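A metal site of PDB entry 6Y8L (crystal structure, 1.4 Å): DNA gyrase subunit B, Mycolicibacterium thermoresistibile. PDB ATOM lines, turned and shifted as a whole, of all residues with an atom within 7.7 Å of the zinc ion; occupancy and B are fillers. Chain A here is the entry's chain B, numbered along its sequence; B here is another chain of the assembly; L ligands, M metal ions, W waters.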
ATOM      1  N   TRP A  30     -18.716  21.264  19.124  1.00  0.00           N
ATOM      2  CA  TRP A  30     -17.855  20.632  18.115  1.00  0.00           C
ATOM      3  C   TRP A  30     -18.081  19.113  18.144  1.00  0.00           C
ATOM      4  O   TRP A  30     -18.109  18.481  17.075  1.00  0.00           O
ATOM      5  CB  TRP A  30     -16.394  21.013  18.330  1.00  0.00           C
ATOM      6  CG  TRP A  30     -16.018  22.428  17.973  1.00  0.00           C
ATOM      7  CD1 TRP A  30     -16.634  23.289  17.124  1.00  0.00           C
ATOM      8  CD2 TRP A  30     -14.905  23.154  18.528  1.00  0.00           C
ATOM      9  NE1 TRP A  30     -15.964  24.488  17.059  1.00  0.00           N
ATOM     10  CE2 TRP A  30     -14.903  24.430  17.919  1.00  0.00           C
ATOM     11  CE3 TRP A  30     -13.863  22.855  19.419  1.00  0.00           C
ATOM     12  CZ2 TRP A  30     -13.932  25.408  18.202  1.00  0.00           C
ATOM     13  CZ3 TRP A  30     -12.898  23.809  19.686  1.00  0.00           C
ATOM     14  CH2 TRP A  30     -12.940  25.070  19.092  1.00  0.00           C
ATOM     15  N   GLU A  31     -18.146  18.513  19.322  1.00  0.00           N
ATOM     16  CA  GLU A  31     -18.270  17.041  19.464  1.00  0.00           C
ATOM     17  C   GLU A  31     -19.616  16.585  18.905  1.00  0.00           C
ATOM     18  O   GLU A  31     -19.656  15.619  18.130  1.00  0.00           O
ATOM     19  CB  GLU A  31     -18.163  16.605  20.917  1.00  0.00           C
ATOM     20  CG  GLU A  31     -18.215  15.111  21.091  1.00  0.00           C
ATOM     21  CD  GLU A  31     -17.042  14.352  20.494  1.00  0.00           C
ATOM     22  OE1 GLU A  31     -15.920  14.860  20.514  1.00  0.00           O
ATOM     23  OE2 GLU A  31     -17.261  13.232  20.067  1.00  0.00           O
ATOM     24  N   VAL A  33     -21.756  18.106  16.869  1.00  0.00           N
ATOM     25  CA  VAL A  33     -21.740  18.335  15.392  1.00  0.00           C
ATOM     26  C   VAL A  33     -20.905  17.245  14.714  1.00  0.00           C
ATOM     27  O   VAL A  33     -21.340  16.687  13.696  1.00  0.00           O
ATOM     28  CB  VAL A  33     -21.239  19.744  15.063  1.00  0.00           C
ATOM     29  CG1 VAL A  33     -20.839  19.886  13.589  1.00  0.00           C
ATOM     30  CG2 VAL A  33     -22.259  20.778  15.505  1.00  0.00           C
ATOM     31  N   ASP A  34     -19.693  17.001  15.201  1.00  0.00           N
ATOM     32  CA  ASP A  34     -18.832  15.973  14.588  1.00  0.00           C
ATOM     33  C   ASP A  34     -19.610  14.650  14.476  1.00  0.00           C
ATOM     34  O   ASP A  34     -19.540  13.980  13.428  1.00  0.00           O
ATOM     35  CB  ASP A  34     -17.568  15.767  15.414  1.00  0.00           C
ATOM     36  CG  ASP A  34     -16.852  14.532  14.930  1.00  0.00           C
ATOM     37  OD1 ASP A  34     -16.153  14.631  13.902  1.00  0.00           O
ATOM     38  OD2 ASP A  34     -17.039  13.488  15.558  1.00  0.00           O
ATOM     39  N   ASN A  35     -20.281  14.268  15.566  1.00  0.00           N
ATOM     40  CA  ASN A  35     -20.896  12.933  15.658  1.00  0.00           C
ATOM     41  C   ASN A  35     -21.977  12.823  14.576  1.00  0.00           C
ATOM     42  O   ASN A  35     -22.148  11.737  13.990  1.00  0.00           O
ATOM     43  CB  ASN A  35     -21.472  12.669  17.043  1.00  0.00           C
ATOM     44  CG  ASN A  35     -20.446  12.579  18.160  1.00  0.00           C
ATOM     45  OD1 ASN A  35     -20.843  12.461  19.312  1.00  0.00           O
ATOM     46  ND2 ASN A  35     -19.127  12.591  17.863  1.00  0.00           N
ATOM     47  N   ALA A  36     -22.719  13.904  14.352  1.00  0.00           N
ATOM     48  CA  ALA A  36     -23.803  13.942  13.347  1.00  0.00           C
ATOM     49  C   ALA A  36     -23.183  13.896  11.956  1.00  0.00           C
ATOM     50  O   ALA A  36     -23.612  13.108  11.084  1.00  0.00           O
ATOM     51  CB  ALA A  36     -24.622  15.202  13.572  1.00  0.00           C
ATOM     52  N   VAL A  37     -22.184  14.723  11.713  1.00  0.00           N
ATOM     53  CA  VAL A  37     -21.539  14.832  10.379  1.00  0.00           C
ATOM     54  C   VAL A  37     -20.897  13.484  10.014  1.00  0.00           C
ATOM     55  O   VAL A  37     -20.944  13.118   8.813  1.00  0.00           O
ATOM     56  CB  VAL A  37     -20.521  15.984  10.320  1.00  0.00           C
ATOM     57  CG1 VAL A  37     -19.724  15.920   9.032  1.00  0.00           C
ATOM     58  CG2 VAL A  37     -21.261  17.334  10.447  1.00  0.00           C
ATOM     59  N   ASP A  38     -20.396  12.750  10.988  1.00  0.00           N
ATOM     60  CA  ASP A  38     -19.803  11.409  10.787  1.00  0.00           C
ATOM     61  C   ASP A  38     -20.789  10.523  10.022  1.00  0.00           C
ATOM     62  O   ASP A  38     -20.365   9.622   9.291  1.00  0.00           O
ATOM     63  CB  ASP A  38     -19.452  10.750  12.107  1.00  0.00           C
ATOM     64  CG  ASP A  38     -18.196  11.271  12.785  1.00  0.00           C
ATOM     65  OD1 ASP A  38     -17.388  11.944  12.105  1.00  0.00           O
ATOM     66  OD2 ASP A  38     -18.035  10.952  13.966  1.00  0.00           O
ATOM     67  N   GLU A  39     -22.095  10.711  10.237  1.00  0.00           N
ATOM     68  CA  GLU A  39     -23.107   9.839   9.591  1.00  0.00           C
ATOM     69  C   GLU A  39     -23.247  10.138   8.107  1.00  0.00           C
ATOM     70  O   GLU A  39     -23.882   9.307   7.417  1.00  0.00           O
ATOM     71  CB  GLU A  39     -24.442   9.943  10.330  1.00  0.00           C
ATOM     72  CG  GLU A  39     -24.412   9.206  11.666  1.00  0.00           C
ATOM     73  CD  GLU A  39     -24.197   7.695  11.481  1.00  0.00           C
ATOM     74  OE1 GLU A  39     -25.127   7.037  10.978  1.00  0.00           O
ATOM     75  OE2 GLU A  39     -23.107   7.181  11.754  1.00  0.00           O
ATOM     76  N   GLY B  14     -15.713   2.757  15.364  1.00  0.00           N
ATOM     77  CA  GLY B  14     -16.733   3.666  14.838  1.00  0.00           C
ATOM     78  C   GLY B  14     -17.444   4.447  15.932  1.00  0.00           C
ATOM     79  O   GLY B  14     -17.943   5.560  15.650  1.00  0.00           O
ATOM     80  N   MET B  15     -17.497   3.893  17.141  1.00  0.00           N
ATOM     81  CA  MET B  15     -18.142   4.579  18.302  1.00  0.00           C
ATOM     82  C   MET B  15     -17.253   5.727  18.788  1.00  0.00           C
ATOM     83  O   MET B  15     -17.760   6.565  19.515  1.00  0.00           O
ATOM     84  CB  MET B  15     -18.367   3.581  19.445  1.00  0.00           C
ATOM     85  CG  MET B  15     -19.408   2.525  19.110  1.00  0.00           C
ATOM     86  SD  MET B  15     -21.026   3.137  19.573  1.00  0.00           S
ATOM     87  CE  MET B  15     -22.220   2.166  18.648  1.00  0.00           C
ATOM     88  N   TYR B  16     -15.969   5.759  18.421  1.00  0.00           N
ATOM     89  CA  TYR B  16     -14.990   6.754  18.897  1.00  0.00           C
ATOM     90  C   TYR B  16     -14.576   7.735  17.786  1.00  0.00           C
ATOM     91  O   TYR B  16     -14.273   8.904  18.134  1.00  0.00           O
ATOM     92  CB  TYR B  16     -13.788   6.030  19.495  1.00  0.00           C
ATOM     93  CG  TYR B  16     -14.132   5.282  20.750  1.00  0.00           C
ATOM     94  CD1 TYR B  16     -14.125   5.906  21.995  1.00  0.00           C
ATOM     95  CD2 TYR B  16     -14.551   3.953  20.684  1.00  0.00           C
ATOM     96  CE1 TYR B  16     -14.458   5.224  23.149  1.00  0.00           C
ATOM     97  CE2 TYR B  16     -14.873   3.251  21.837  1.00  0.00           C
ATOM     98  CZ  TYR B  16     -14.850   3.896  23.070  1.00  0.00           C
ATOM     99  OH  TYR B  16     -15.184   3.200  24.180  1.00  0.00           O
ATOM    100  N   ILE B  17     -14.507   7.280  16.533  1.00  0.00           N
ATOM    101  CA  ILE B  17     -14.038   8.113  15.403  1.00  0.00           C
ATOM    102  C   ILE B  17     -14.965   8.044  14.188  1.00  0.00           C
ATOM    103  O   ILE B  17     -14.581   8.553  13.132  1.00  0.00           O
ATOM    104  CB  ILE B  17     -12.604   7.736  15.021  1.00  0.00           C
ATOM    105  CG1 ILE B  17     -12.478   6.271  14.605  1.00  0.00           C
ATOM    106  CG2 ILE B  17     -11.654   8.067  16.160  1.00  0.00           C
ATOM    107  CD1 ILE B  17     -11.200   5.999  13.851  1.00  0.00           C
ATOM    108  N   GLY B  18     -16.177   7.486  14.366  1.00  0.00           N
ATOM    109  CA  GLY B  18     -17.227   7.519  13.343  1.00  0.00           C
ATOM    110  C   GLY B  18     -17.113   6.394  12.348  1.00  0.00           C
ATOM    111  O   GLY B  18     -18.145   5.826  11.994  1.00  0.00           O
ATOM    112  N   SER B  19     -15.916   6.086  11.886  1.00  0.00           N
ATOM    113  CA  SER B  19     -15.661   5.100  10.812  1.00  0.00           C
ATOM    114  C   SER B  19     -14.161   4.914  10.690  1.00  0.00           C
ATOM    115  O   SER B  19     -13.391   5.626  11.392  1.00  0.00           O
ATOM    116  CB  SER B  19     -16.250   5.520   9.495  1.00  0.00           C
ATOM    117  OG  SER B  19     -15.435   6.517   8.926  1.00  0.00           O
ATOM    118  N   ARG B  23     -11.996   9.922   6.867  1.00  0.00           N
ATOM    119  CA  ARG B  23     -12.507  10.823   7.915  1.00  0.00           C
ATOM    120  C   ARG B  23     -12.137  10.286   9.292  1.00  0.00           C
ATOM    121  O   ARG B  23     -11.769  11.100  10.159  1.00  0.00           O
ATOM    122  CB  ARG B  23     -14.021  10.997   7.787  1.00  0.00           C
ATOM    123  CG  ARG B  23     -14.621  11.940   8.819  1.00  0.00           C
ATOM    124  CD  ARG B  23     -16.096  12.158   8.611  1.00  0.00           C
ATOM    125  NE  ARG B  23     -16.594  12.965   9.704  1.00  0.00           N
ATOM    126  CZ  ARG B  23     -16.535  14.296   9.771  1.00  0.00           C
ATOM    127  NH1 ARG B  23     -16.105  15.021   8.751  1.00  0.00           N
ATOM    128  NH2 ARG B  23     -16.978  14.896  10.868  1.00  0.00           N
ATOM    129  N   GLY B  24     -12.230   8.976   9.531  1.00  0.00           N
ATOM    130  CA  GLY B  24     -11.815   8.359  10.804  1.00  0.00           C
ATOM    131  C   GLY B  24     -10.341   8.646  11.064  1.00  0.00           C
ATOM    132  O   GLY B  24      -9.997   9.080  12.194  1.00  0.00           O
ATOM    133  N   HIS B  27      -9.692  12.050  12.397  1.00  0.00           N
ATOM    134  CA  HIS B  27     -10.058  12.304  13.825  1.00  0.00           C
ATOM    135  C   HIS B  27      -8.776  12.336  14.666  1.00  0.00           C
ATOM    136  O   HIS B  27      -8.721  13.084  15.643  1.00  0.00           O
ATOM    137  CB  HIS B  27     -10.992  11.225  14.354  1.00  0.00           C
ATOM    138  CG  HIS B  27     -12.445  11.418  14.019  1.00  0.00           C
ATOM    139  ND1 HIS B  27     -12.938  11.451  12.739  1.00  0.00           N
ATOM    140  CD2 HIS B  27     -13.506  11.572  14.856  1.00  0.00           C
ATOM    141  CE1 HIS B  27     -14.253  11.588  12.787  1.00  0.00           C
ATOM    142  NE2 HIS B  27     -14.637  11.660  14.079  1.00  0.00           N
ATOM    143  N   TRP B  30      -6.970  15.626  14.172  1.00  0.00           N
ATOM    144  CA  TRP B  30      -7.807  16.713  14.727  1.00  0.00           C
ATOM    145  C   TRP B  30      -7.617  16.752  16.246  1.00  0.00           C
ATOM    146  O   TRP B  30      -7.561  17.860  16.815  1.00  0.00           O
ATOM    147  CB  TRP B  30      -9.280  16.526  14.306  1.00  0.00           C
ATOM    148  CG  TRP B  30      -9.594  16.754  12.850  1.00  0.00           C
ATOM    149  CD1 TRP B  30      -8.934  17.571  11.983  1.00  0.00           C
ATOM    150  CD2 TRP B  30     -10.689  16.194  12.080  1.00  0.00           C
ATOM    151  NE1 TRP B  30      -9.523  17.561  10.737  1.00  0.00           N
ATOM    152  CE2 TRP B  30     -10.602  16.722  10.780  1.00  0.00           C
ATOM    153  CE3 TRP B  30     -11.751  15.324  12.332  1.00  0.00           C
ATOM    154  CZ2 TRP B  30     -11.528  16.444   9.761  1.00  0.00           C
ATOM    155  CZ3 TRP B  30     -12.654  14.995  11.327  1.00  0.00           C
ATOM    156  CH2 TRP B  30     -12.525  15.542  10.049  1.00  0.00           C
HETATM  157  C1  LIG L   1     -23.524  10.177  19.535  1.00  0.00           C
HETATM  158  O1  LIG L   1     -23.530   8.889  18.905  1.00  0.00           O
HETATM  159  N1  LIG L   1     -25.352  11.594  15.607  1.00  0.00           N
HETATM  160  C2  LIG L   1     -24.894  10.332  15.597  1.00  0.00           C
HETATM  161  O2  LIG L   1     -25.312   9.409  14.911  1.00  0.00           O
HETATM  162  O3  LIG L   1     -23.820  10.194  16.378  1.00  0.00           O
HETATM  163  C3  LIG L   1     -22.596   8.712  17.851  1.00  0.00           C
HETATM  164  C4  LIG L   1     -23.267   8.875  16.495  1.00  0.00           C
HETATM  165  C5  LIG L   1     -22.242   8.677  15.388  1.00  0.00           C
HETATM  166  O4  LIG L   1     -21.185   9.639  15.416  1.00  0.00           O
HETATM  167  C6  LIG L   1     -21.663   7.273  15.531  1.00  0.00           C
HETATM  168  O5  LIG L   1     -21.134   7.036  16.829  1.00  0.00           O
HETATM  169  C7  LIG L   1     -21.955   7.328  17.994  1.00  0.00           C
HETATM  170  C8  LIG L   1     -22.987   6.217  18.165  1.00  0.00           C
HETATM  171  C9  LIG L   1     -20.993   7.296  19.164  1.00  0.00           C
HETATM  172  O6  LIG L   1     -22.751   6.407  15.267  1.00  0.00           O
HETATM  173  C10 LIG L   1     -22.561   5.050  15.042  1.00  0.00           C
HETATM  174  C11 LIG L   1     -23.698   4.378  14.572  1.00  0.00           C
HETATM  175  C12 LIG L   1     -25.012   5.075  14.407  1.00  0.00           C
HETATM  176  C13 LIG L   1     -23.570   3.029  14.307  1.00  0.00           C
HETATM  177  C14 LIG L   1     -22.381   2.339  14.444  1.00  0.00           C
HETATM  178  C15 LIG L   1     -21.256   3.042  14.899  1.00  0.00           C
HETATM  179  C16 LIG L   1     -21.329   4.376  15.165  1.00  0.00           C
HETATM  180  O7  LIG L   1     -24.708   2.394  13.886  1.00  0.00           O
HETATM  181  C17 LIG L   1     -24.735   1.060  13.526  1.00  0.00           C
HETATM  182  O8  LIG L   1     -25.799   0.620  13.163  1.00  0.00           O
HETATM  183  C18 LIG L   1     -23.576   0.310  13.673  1.00  0.00           C
HETATM  184  C19 LIG L   1     -22.398   0.940  14.125  1.00  0.00           C
HETATM  185  O9  LIG L   1     -21.246   0.261  14.247  1.00  0.00           O
HETATM  186  N2  LIG L   1     -23.594  -1.055  13.304  1.00  0.00           N
HETATM  187  C20 LIG L   1     -24.147  -2.130  13.933  1.00  0.00           C
HETATM  188  O10 LIG L   1     -24.319  -3.209  13.376  1.00  0.00           O
HETATM  189  C21 LIG L   1     -24.397  -1.997  15.396  1.00  0.00           C
HETATM  190  C22 LIG L   1     -23.352  -1.627  16.233  1.00  0.00           C
HETATM  191  C23 LIG L   1     -23.512  -1.539  17.614  1.00  0.00           C
HETATM  192  C24 LIG L   1     -24.773  -1.844  18.145  1.00  0.00           C
HETATM  193  O11 LIG L   1     -24.975  -1.769  19.495  1.00  0.00           O
HETATM  194  C25 LIG L   1     -25.806  -2.245  17.324  1.00  0.00           C
HETATM  195  C26 LIG L   1     -25.632  -2.311  15.969  1.00  0.00           C
HETATM  196  C27 LIG L   1     -22.346  -1.127  18.487  1.00  0.00           C
HETATM  197  C28 LIG L   1     -21.076  -1.879  18.181  1.00  0.00           C
HETATM  198  C29 LIG L   1     -20.162  -1.605  17.252  1.00  0.00           C
HETATM  199  C30 LIG L   1     -19.301  -2.679  16.644  1.00  0.00           C
HETATM  200  C31 LIG L   1     -19.877  -0.210  16.739  1.00  0.00           C
HETATM  201 ZN    ZN M   1     -16.486  11.784  14.785  1.00  0.00          ZN
HETATM  202  O   HOH W   1     -16.488  10.574  16.383  1.00  0.00           O
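The backbone carbonyl oxygen (O) of Asn 35 lies within hydrogen-bond range of an oxygen (O4) of the ligand, at 2.7 Å.
OD1 of Asp 38 is in salt-bridge range of NE of Arg 23 of chain B, 2.7 Å away. The side-chain amide nitrogen (ND2) of Asn 35 sits close to the side-chain carboxylate (OD2) of Asp 34. NH2 of Arg 23 of chain B is in salt-bridge range of OD1 of Asp 34, 3.2 Å away. ND1 of His 27 of chain B lies close to O of Ile 17 of chain B (3.4 Å). A ring nitrogen (ND1) of His 27 of chain B sits at hydrogen-bond distance from the backbone carbonyl oxygen of Arg 23 of chain B, 2.9 Å away.
Within 4 Å of the zinc ion: Asp 34, Asp 38 and His 27 of chain B. The nearest printed residue that does not touch the zinc ion is Ile 17 of chain B (4.1 Å).
OD2 of Asp 38 binds the zinc ion (1.9 Å). OD2 of Asp 34 binds the zinc ion, at 2.0 Å. NE2 of His 27 of chain B binds the zinc ion, 2.0 Å away. Water W1 is bound to the zinc ion. The zinc ion has four donor atoms within binding distance. Slightly farther from the zinc ion lies OD1 of Asp 38 (2.8 Å).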
